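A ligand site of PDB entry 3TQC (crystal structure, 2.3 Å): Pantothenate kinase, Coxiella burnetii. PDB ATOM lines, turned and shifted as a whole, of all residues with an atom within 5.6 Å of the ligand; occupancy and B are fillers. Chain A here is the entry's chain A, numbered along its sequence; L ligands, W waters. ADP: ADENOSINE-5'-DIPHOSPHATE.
O of Ile 49 lies close to N1 of the ligand (3.5 Å). O of Ser 100 sits close to O2B of the ligand (3.4 Å). Val 50 touches the ligand. OH of Tyr 59 touches N6 of the ligand, 3.9 Å away. Val 101 touches the ligand (C to O3B, 3.9 Å). Hydrophobic or aromatic side chains within 4 Å of the ligand: Ile 49, Val 50 and His 311. 14 residues have an atom within 4 Å of the ligand: Ile 49, Val 50, Tyr 59, Ser 100, Val 101, Ala 102, Val 103, Gly 104, Lys 105, Ser 106, Thr 107, Arg 247, Lys 307 and His 311.
The backbone carbonyl oxygen of Ser 100 sits at hydrogen-bond distance from the side-chain amino group of Lys 105, 2.8 Å away. The backbone carbonyl oxygen of Arg 247 lies within hydrogen-bond range of the side-chain hydroxyl of Ser 250 (2.8 Å). NH2 of Arg 110 sits at hydrogen-bond distance from OG of Ser 106, 2.8 Å away. The side-chain hydroxyl (OG1) of Thr 108 is in hydrogen-bond range of the backbone carbonyl oxygen (O) of Gly 104 (2.9 Å). A ring nitrogen (ND1) of His 311 sits at hydrogen-bond distance from the side-chain amino group (NZ) of Lys 307, 3.0 Å away. A ring nitrogen (NE2) of His 311 sits at hydrogen-bond distance from the indole nitrogen (NE1) of Trp 243. O of Val 103 lies within hydrogen-bond range of NZ of Lys 307 (2.9 Å). N of Tyr 59 is in hydrogen-bond range of O of Glu 54.
Water W6 bridges the backbone carbonyl oxygen (O) of Val 50 (2.6 Å) and a nitrogen (N1) of the ligand (2.6 Å). Water W5 lies within hydrogen-bond range of O of Trp 243 (2.6 Å), O3' of the ligand (2.8 Å) and N of Arg 247 (3.4 Å). Water W1 lies within hydrogen-bond range of the side-chain amino group of Lys 307 (2.8 Å), a nitrogen (N6) of the ligand (2.9 Å), the side-chain hydroxyl of Thr 108 (3.0 Å) and the side-chain hydroxyl of Tyr 59 (3.2 Å). Water W4 lies within hydrogen-bond range of the side-chain hydroxyl of Tyr 59 (2.6 Å), the backbone carbonyl oxygen of His 311 (2.6 Å), the side-chain carboxylate of Glu 54 (2.7 Å) and a nitrogen (N6) of the ligand (3.1 Å). Water W3 bridges the side-chain amino group of Lys 105 (3.0 Å) and an oxygen (O3B) of the ligand (3.3 Å).
An oxygen (O2B) of the ligand is in hydrogen-bond range of the backbone NH (N) of Lys 105 (2.8 Å). NZ of Lys 105 lies within salt-bridge range of O2B of the ligand (2.7 Å). An oxygen (O1A) of the ligand sits at hydrogen-bond distance from the backbone NH of Thr 107, 2.8 Å away. An oxygen (O1A) of the ligand lies within hydrogen-bond range of the side-chain hydroxyl (OG1) of Thr 107, at 2.8 Å. The guanidinium group (NH1) of Arg 247 is in salt-bridge range of an oxygen (O3B) of the ligand (2.8 Å). The backbone NH (N) of Ser 106 sits at hydrogen-bond distance from an oxygen (O1B) of the ligand, at 2.8 Å. The backbone NH of Ala 102 sits at hydrogen-bond distance from an oxygen (O3B) of the ligand (2.9 Å). The backbone NH (N) of Gly 104 sits at hydrogen-bond distance from an oxygen (O3A) of the ligand (3.1 Å). NE2 of His 311 lies close to N3 of the ligand, 3.4 Å away. The side-chain amino group of Lys 307 is in hydrogen-bond range of a nitrogen (N7) of the ligand, 3.2 Å away. The backbone NH of Val 103 lies within hydrogen-bond range of an oxygen (O2B) of the ligand (3.4 Å).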
ATOM      1  N   ILE A  49       0.413 -14.184   0.294  1.00  0.00           N
ATOM      2  CA  ILE A  49       1.046 -12.952  -0.136  1.00  0.00           C
ATOM      3  C   ILE A  49       0.130 -11.755   0.068  1.00  0.00           C
ATOM      4  O   ILE A  49       0.559 -10.755   0.611  1.00  0.00           O
ATOM      5  CB  ILE A  49       1.455 -13.025  -1.638  1.00  0.00           C
ATOM      6  CG1 ILE A  49       2.659 -13.955  -1.821  1.00  0.00           C
ATOM      7  CG2 ILE A  49       1.776 -11.657  -2.163  1.00  0.00           C
ATOM      8  CD1 ILE A  49       2.859 -14.392  -3.284  1.00  0.00           C
ATOM      9  N   VAL A  50      -1.110 -11.848  -0.400  1.00  0.00           N
ATOM     10  CA  VAL A  50      -2.031 -10.716  -0.389  1.00  0.00           C
ATOM     11  C   VAL A  50      -2.802 -10.540   0.933  1.00  0.00           C
ATOM     12  O   VAL A  50      -3.114  -9.420   1.306  1.00  0.00           O
ATOM     13  CB  VAL A  50      -3.029 -10.782  -1.550  1.00  0.00           C
ATOM     14  CG1 VAL A  50      -3.966  -9.577  -1.521  1.00  0.00           C
ATOM     15  CG2 VAL A  50      -2.299 -10.861  -2.890  1.00  0.00           C
ATOM     16  N   GLU A  54      -7.351  -8.550   2.747  1.00  0.00           N
ATOM     17  CA  GLU A  54      -7.277  -7.758   1.545  1.00  0.00           C
ATOM     18  C   GLU A  54      -8.044  -8.398   0.394  1.00  0.00           C
ATOM     19  O   GLU A  54      -8.667  -7.697  -0.412  1.00  0.00           O
ATOM     20  CB  GLU A  54      -5.821  -7.561   1.155  1.00  0.00           C
ATOM     21  CG  GLU A  54      -5.602  -6.604   0.020  1.00  0.00           C
ATOM     22  CD  GLU A  54      -5.749  -5.138   0.400  1.00  0.00           C
ATOM     23  OE1 GLU A  54      -6.120  -4.813   1.545  1.00  0.00           O
ATOM     24  OE2 GLU A  54      -5.488  -4.313  -0.477  1.00  0.00           O
ATOM     25  N   TYR A  59     -10.373  -7.261  -3.331  1.00  0.00           N
ATOM     26  CA  TYR A  59     -10.434  -7.967  -4.614  1.00  0.00           C
ATOM     27  C   TYR A  59     -11.744  -8.718  -4.823  1.00  0.00           C
ATOM     28  O   TYR A  59     -12.196  -8.838  -5.940  1.00  0.00           O
ATOM     29  CB  TYR A  59      -9.205  -8.871  -4.824  1.00  0.00           C
ATOM     30  CG  TYR A  59      -7.945  -8.041  -4.805  1.00  0.00           C
ATOM     31  CD1 TYR A  59      -7.573  -7.297  -5.898  1.00  0.00           C
ATOM     32  CD2 TYR A  59      -7.188  -7.939  -3.648  1.00  0.00           C
ATOM     33  CE1 TYR A  59      -6.445  -6.501  -5.866  1.00  0.00           C
ATOM     34  CE2 TYR A  59      -6.073  -7.147  -3.596  1.00  0.00           C
ATOM     35  CZ  TYR A  59      -5.697  -6.426  -4.707  1.00  0.00           C
ATOM     36  OH  TYR A  59      -4.572  -5.645  -4.641  1.00  0.00           O
ATOM     37  N   GLY A  99       0.815  -1.041 -14.838  1.00  0.00           N
ATOM     38  CA  GLY A  99       1.533  -0.454 -13.729  1.00  0.00           C
ATOM     39  C   GLY A  99       3.014  -0.751 -13.803  1.00  0.00           C
ATOM     40  O   GLY A  99       3.441  -1.530 -14.625  1.00  0.00           O
ATOM     41  N   SER A 100       3.779  -0.118 -12.919  1.00  0.00           N
ATOM     42  CA  SER A 100       5.220  -0.297 -12.858  1.00  0.00           C
ATOM     43  C   SER A 100       5.619  -1.734 -12.684  1.00  0.00           C
ATOM     44  O   SER A 100       4.834  -2.563 -12.210  1.00  0.00           O
ATOM     45  CB  SER A 100       5.791   0.499 -11.688  1.00  0.00           C
ATOM     46  OG  SER A 100       7.142   0.185 -11.446  1.00  0.00           O
ATOM     47  N   VAL A 101       6.855  -2.044 -13.055  1.00  0.00           N
ATOM     48  CA  VAL A 101       7.484  -3.290 -12.648  1.00  0.00           C
ATOM     49  C   VAL A 101       7.414  -3.346 -11.120  1.00  0.00           C
ATOM     50  O   VAL A 101       7.678  -2.334 -10.468  1.00  0.00           O
ATOM     51  CB  VAL A 101       8.946  -3.340 -13.084  1.00  0.00           C
ATOM     52  CG1 VAL A 101       9.644  -4.597 -12.566  1.00  0.00           C
ATOM     53  CG2 VAL A 101       9.075  -3.223 -14.626  1.00  0.00           C
ATOM     54  N   ALA A 102       7.024  -4.501 -10.570  1.00  0.00           N
ATOM     55  CA  ALA A 102       7.014  -4.756  -9.136  1.00  0.00           C
ATOM     56  C   ALA A 102       5.857  -4.072  -8.358  1.00  0.00           C
ATOM     57  O   ALA A 102       5.853  -4.078  -7.121  1.00  0.00           O
ATOM     58  CB  ALA A 102       8.369  -4.371  -8.522  1.00  0.00           C
ATOM     59  N   VAL A 103       4.893  -3.480  -9.057  1.00  0.00           N
ATOM     60  CA  VAL A 103       3.805  -2.809  -8.392  1.00  0.00           C
ATOM     61  C   VAL A 103       2.737  -3.817  -7.968  1.00  0.00           C
ATOM     62  O   VAL A 103       1.870  -3.514  -7.148  1.00  0.00           O
ATOM     63  CB  VAL A 103       3.180  -1.712  -9.292  1.00  0.00           C
ATOM     64  CG1 VAL A 103       2.135  -2.307 -10.220  1.00  0.00           C
ATOM     65  CG2 VAL A 103       2.555  -0.617  -8.440  1.00  0.00           C
ATOM     66  N   GLY A 104       2.792  -5.018  -8.538  1.00  0.00           N
ATOM     67  CA  GLY A 104       1.857  -6.076  -8.198  1.00  0.00           C
ATOM     68  C   GLY A 104       0.893  -6.477  -9.288  1.00  0.00           C
ATOM     69  O   GLY A 104      -0.137  -7.072  -9.016  1.00  0.00           O
ATOM     70  N   LYS A 105       1.227  -6.169 -10.537  1.00  0.00           N
ATOM     71  CA  LYS A 105       0.373  -6.541 -11.671  1.00  0.00           C
ATOM     72  C   LYS A 105       0.072  -8.030 -11.686  1.00  0.00           C
ATOM     73  O   LYS A 105      -1.090  -8.441 -11.754  1.00  0.00           O
ATOM     74  CB  LYS A 105       1.040  -6.174 -12.985  1.00  0.00           C
ATOM     75  CG  LYS A 105       1.099  -4.687 -13.248  1.00  0.00           C
ATOM     76  CD  LYS A 105       1.544  -4.410 -14.678  1.00  0.00           C
ATOM     77  CE  LYS A 105       2.938  -4.950 -14.952  1.00  0.00           C
ATOM     78  NZ  LYS A 105       3.873  -4.597 -13.875  1.00  0.00           N
ATOM     79  N   SER A 106       1.122  -8.836 -11.622  1.00  0.00           N
ATOM     80  CA  SER A 106       0.979 -10.275 -11.713  1.00  0.00           C
ATOM     81  C   SER A 106       0.141 -10.821 -10.553  1.00  0.00           C
ATOM     82  O   SER A 106      -0.741 -11.662 -10.731  1.00  0.00           O
ATOM     83  CB  SER A 106       2.357 -10.921 -11.728  1.00  0.00           C
ATOM     84  OG  SER A 106       2.236 -12.326 -11.840  1.00  0.00           O
ATOM     85  N   THR A 107       0.397 -10.316  -9.347  1.00  0.00           N
ATOM     86  CA  THR A 107      -0.340 -10.755  -8.185  1.00  0.00           C
ATOM     87  C   THR A 107      -1.807 -10.412  -8.328  1.00  0.00           C
ATOM     88  O   THR A 107      -2.676 -11.229  -8.066  1.00  0.00           O
ATOM     89  CB  THR A 107       0.229 -10.112  -6.937  1.00  0.00           C
ATOM     90  OG1 THR A 107       1.628 -10.445  -6.838  1.00  0.00           O
ATOM     91  CG2 THR A 107      -0.514 -10.581  -5.707  1.00  0.00           C
ATOM     92  N   THR A 108      -2.081  -9.196  -8.764  1.00  0.00           N
ATOM     93  CA  THR A 108      -3.453  -8.728  -8.929  1.00  0.00           C
ATOM     94  C   THR A 108      -4.158  -9.566  -9.979  1.00  0.00           C
ATOM     95  O   THR A 108      -5.296  -9.961  -9.803  1.00  0.00           O
ATOM     96  CB  THR A 108      -3.500  -7.232  -9.308  1.00  0.00           C
ATOM     97  OG1 THR A 108      -2.860  -6.468  -8.277  1.00  0.00           O
ATOM     98  CG2 THR A 108      -4.909  -6.759  -9.472  1.00  0.00           C
ATOM     99  N   ARG A 110      -3.516 -12.635 -10.797  1.00  0.00           N
ATOM    100  CA  ARG A 110      -3.786 -13.997 -10.316  1.00  0.00           C
ATOM    101  C   ARG A 110      -4.959 -14.007  -9.369  1.00  0.00           C
ATOM    102  O   ARG A 110      -5.781 -14.919  -9.414  1.00  0.00           O
ATOM    103  CB  ARG A 110      -2.563 -14.620  -9.651  1.00  0.00           C
ATOM    104  CG  ARG A 110      -1.543 -15.184 -10.642  1.00  0.00           C
ATOM    105  CD  ARG A 110      -0.445 -15.984  -9.912  1.00  0.00           C
ATOM    106  NE  ARG A 110       0.627 -15.088  -9.467  1.00  0.00           N
ATOM    107  CZ  ARG A 110       1.739 -14.827 -10.161  1.00  0.00           C
ATOM    108  NH1 ARG A 110       1.968 -15.402 -11.348  1.00  0.00           N
ATOM    109  NH2 ARG A 110       2.643 -13.971  -9.655  1.00  0.00           N
ATOM    110  N   GLU A 203      -2.035  -8.559 -18.665  1.00  0.00           N
ATOM    111  CA  GLU A 203      -1.190  -7.760 -17.794  1.00  0.00           C
ATOM    112  C   GLU A 203       0.131  -7.428 -18.432  1.00  0.00           C
ATOM    113  O   GLU A 203       0.751  -8.258 -19.115  1.00  0.00           O
ATOM    114  CB  GLU A 203      -0.974  -8.441 -16.455  1.00  0.00           C
ATOM    115  CG  GLU A 203      -0.371  -9.795 -16.534  1.00  0.00           C
ATOM    116  CD  GLU A 203       0.726  -9.986 -15.531  1.00  0.00           C
ATOM    117  OE1 GLU A 203       1.488  -9.025 -15.301  1.00  0.00           O
ATOM    118  OE2 GLU A 203       0.852 -11.111 -15.000  1.00  0.00           O
ATOM    119  N   TRP A 243       9.519  -2.730  -2.843  1.00  0.00           N
ATOM    120  CA  TRP A 243       8.942  -4.001  -3.257  1.00  0.00           C
ATOM    121  C   TRP A 243       9.818  -4.712  -4.290  1.00  0.00           C
ATOM    122  O   TRP A 243       9.899  -5.944  -4.299  1.00  0.00           O
ATOM    123  CB  TRP A 243       7.541  -3.818  -3.832  1.00  0.00           C
ATOM    124  CG  TRP A 243       6.570  -3.178  -2.893  1.00  0.00           C
ATOM    125  CD1 TRP A 243       6.656  -3.120  -1.522  1.00  0.00           C
ATOM    126  CD2 TRP A 243       5.371  -2.519  -3.258  1.00  0.00           C
ATOM    127  NE1 TRP A 243       5.572  -2.436  -1.018  1.00  0.00           N
ATOM    128  CE2 TRP A 243       4.758  -2.066  -2.069  1.00  0.00           C
ATOM    129  CE3 TRP A 243       4.737  -2.247  -4.486  1.00  0.00           C
ATOM    130  CZ2 TRP A 243       3.555  -1.372  -2.059  1.00  0.00           C
ATOM    131  CZ3 TRP A 243       3.557  -1.557  -4.481  1.00  0.00           C
ATOM    132  CH2 TRP A 243       2.976  -1.111  -3.276  1.00  0.00           C
ATOM    133  N   ASP A 246      12.982  -5.946  -2.587  1.00  0.00           N
ATOM    134  CA  ASP A 246      12.564  -7.095  -1.791  1.00  0.00           C
ATOM    135  C   ASP A 246      12.240  -8.328  -2.634  1.00  0.00           C
ATOM    136  O   ASP A 246      12.574  -9.445  -2.227  1.00  0.00           O
ATOM    137  CB  ASP A 246      11.403  -6.726  -0.861  1.00  0.00           C
ATOM    138  CG  ASP A 246      11.865  -5.835   0.295  1.00  0.00           C
ATOM    139  OD1 ASP A 246      13.055  -5.888   0.659  1.00  0.00           O
ATOM    140  OD2 ASP A 246      11.046  -5.086   0.840  1.00  0.00           O
ATOM    141  N   ARG A 247      11.643  -8.135  -3.801  1.00  0.00           N
ATOM    142  CA  ARG A 247      11.378  -9.263  -4.697  1.00  0.00           C
ATOM    143  C   ARG A 247      12.689  -9.894  -5.184  1.00  0.00           C
ATOM    144  O   ARG A 247      12.828 -11.125  -5.164  1.00  0.00           O
ATOM    145  CB  ARG A 247      10.554  -8.847  -5.905  1.00  0.00           C
ATOM    146  CG  ARG A 247      10.126 -10.038  -6.758  1.00  0.00           C
ATOM    147  CD  ARG A 247       9.236  -9.594  -7.886  1.00  0.00           C
ATOM    148  NE  ARG A 247       9.933  -8.806  -8.896  1.00  0.00           N
ATOM    149  CZ  ARG A 247       9.336  -8.222  -9.939  1.00  0.00           C
ATOM    150  NH1 ARG A 247       8.018  -8.324 -10.122  1.00  0.00           N
ATOM    151  NH2 ARG A 247      10.075  -7.536 -10.811  1.00  0.00           N
ATOM    152  N   SER A 250      14.194 -11.730  -2.401  1.00  0.00           N
ATOM    153  CA  SER A 250      13.494 -12.992  -2.126  1.00  0.00           C
ATOM    154  C   SER A 250      13.973 -14.081  -3.081  1.00  0.00           C
ATOM    155  O   SER A 250      14.196 -15.222  -2.655  1.00  0.00           O
ATOM    156  CB  SER A 250      11.970 -12.824  -2.207  1.00  0.00           C
ATOM    157  OG  SER A 250      11.509 -13.021  -3.537  1.00  0.00           O
ATOM    158  N   LYS A 307      -2.125   1.801  -4.020  1.00  0.00           N
ATOM    159  CA  LYS A 307      -1.608   0.983  -2.927  1.00  0.00           C
ATOM    160  C   LYS A 307      -0.769   1.795  -1.960  1.00  0.00           C
ATOM    161  O   LYS A 307      -0.041   2.680  -2.356  1.00  0.00           O
ATOM    162  CB  LYS A 307      -0.785  -0.179  -3.488  1.00  0.00           C
ATOM    163  CG  LYS A 307      -1.652  -1.236  -4.155  1.00  0.00           C
ATOM    164  CD  LYS A 307      -0.853  -2.282  -4.915  1.00  0.00           C
ATOM    165  CE  LYS A 307      -0.034  -3.188  -4.034  1.00  0.00           C
ATOM    166  NZ  LYS A 307       0.418  -4.419  -4.802  1.00  0.00           N
ATOM    167  N   ASP A 310       2.396  -0.992   2.369  1.00  0.00           N
ATOM    168  CA  ASP A 310       2.227  -2.386   2.799  1.00  0.00           C
ATOM    169  C   ASP A 310       1.392  -3.183   1.798  1.00  0.00           C
ATOM    170  O   ASP A 310       0.910  -4.275   2.120  1.00  0.00           O
ATOM    171  CB  ASP A 310       1.588  -2.446   4.204  1.00  0.00           C
ATOM    172  CG  ASP A 310       0.161  -1.870   4.248  1.00  0.00           C
ATOM    173  OD1 ASP A 310      -0.351  -1.376   3.224  1.00  0.00           O
ATOM    174  OD2 ASP A 310      -0.457  -1.905   5.335  1.00  0.00           O
ATOM    175  N   HIS A 311       1.217  -2.629   0.595  1.00  0.00           N
ATOM    176  CA  HIS A 311       0.364  -3.202  -0.479  1.00  0.00           C
ATOM    177  C   HIS A 311      -1.175  -3.054  -0.313  1.00  0.00           C
ATOM    178  O   HIS A 311      -1.930  -3.346  -1.266  1.00  0.00           O
ATOM    179  CB  HIS A 311       0.688  -4.677  -0.711  1.00  0.00           C
ATOM    180  CG  HIS A 311       2.069  -4.912  -1.257  1.00  0.00           C
ATOM    181  ND1 HIS A 311       2.366  -4.789  -2.591  1.00  0.00           N
ATOM    182  CD2 HIS A 311       3.215  -5.283  -0.633  1.00  0.00           C
ATOM    183  CE1 HIS A 311       3.638  -5.082  -2.781  1.00  0.00           C
ATOM    184  NE2 HIS A 311       4.185  -5.363  -1.611  1.00  0.00           N
HETATM  185  PB  ADP L   1       4.601  -7.064 -11.187  1.00  0.00           P
HETATM  186  O1B ADP L   1       3.865  -8.236 -11.744  1.00  0.00           O
HETATM  187  O2B ADP L   1       3.879  -5.747 -11.412  1.00  0.00           O
HETATM  188  O3B ADP L   1       6.066  -6.990 -11.583  1.00  0.00           O
HETATM  189  PA  ADP L   1       4.339  -8.678  -8.753  1.00  0.00           P
HETATM  190  O1A ADP L   1       2.910  -9.103  -8.896  1.00  0.00           O
HETATM  191  O2A ADP L   1       5.434  -9.678  -9.004  1.00  0.00           O
HETATM  192  O3A ADP L   1       4.595  -7.288  -9.580  1.00  0.00           O
HETATM  193  O5' ADP L   1       4.553  -8.242  -7.245  1.00  0.00           O
HETATM  194  C5' ADP L   1       5.700  -7.504  -6.861  1.00  0.00           C
HETATM  195  C4' ADP L   1       6.087  -7.861  -5.436  1.00  0.00           C
HETATM  196  O4' ADP L   1       5.092  -7.356  -4.544  1.00  0.00           O
HETATM  197  C3' ADP L   1       6.125  -9.369  -5.254  1.00  0.00           C
HETATM  198  O3' ADP L   1       7.141  -9.708  -4.310  1.00  0.00           O
HETATM  199  C2' ADP L   1       4.769  -9.699  -4.675  1.00  0.00           C
HETATM  200  O2' ADP L   1       4.886 -10.836  -3.839  1.00  0.00           O
HETATM  201  C1' ADP L   1       4.411  -8.435  -3.894  1.00  0.00           C
HETATM  202  N9  ADP L   1       2.987  -8.114  -3.886  1.00  0.00           N
HETATM  203  C8  ADP L   1       2.257  -7.809  -4.983  1.00  0.00           C
HETATM  204  N7  ADP L   1       0.979  -7.540  -4.651  1.00  0.00           N
HETATM  205  C5  ADP L   1       0.884  -7.680  -3.330  1.00  0.00           C
HETATM  206  C6  ADP L   1      -0.211  -7.522  -2.366  1.00  0.00           C
HETATM  207  N6  ADP L   1      -1.441  -7.173  -2.836  1.00  0.00           N
HETATM  208  N1  ADP L   1       0.065  -7.747  -1.067  1.00  0.00           N
HETATM  209  C2  ADP L   1       1.317  -8.080  -0.644  1.00  0.00           C
HETATM  210  N3  ADP L   1       2.374  -8.232  -1.481  1.00  0.00           N
HETATM  211  C4  ADP L   1       2.209  -8.041  -2.809  1.00  0.00           C
HETATM  212  O   HOH W   1      -1.533  -6.261  -5.552  1.00  0.00           O
HETATM  213  O   HOH W   2       5.958 -11.054  -1.432  1.00  0.00           O
HETATM  214  O   HOH W   3       6.358  -6.111 -14.756  1.00  0.00           O
HETATM  215  O   HOH W   4      -3.661  -5.018  -2.277  1.00  0.00           O
HETATM  216  O   HOH W   5       8.401  -7.576  -2.912  1.00  0.00           O
HETATM  217  O   HOH W   6      -1.903  -7.187   0.607  1.00  0.00           O
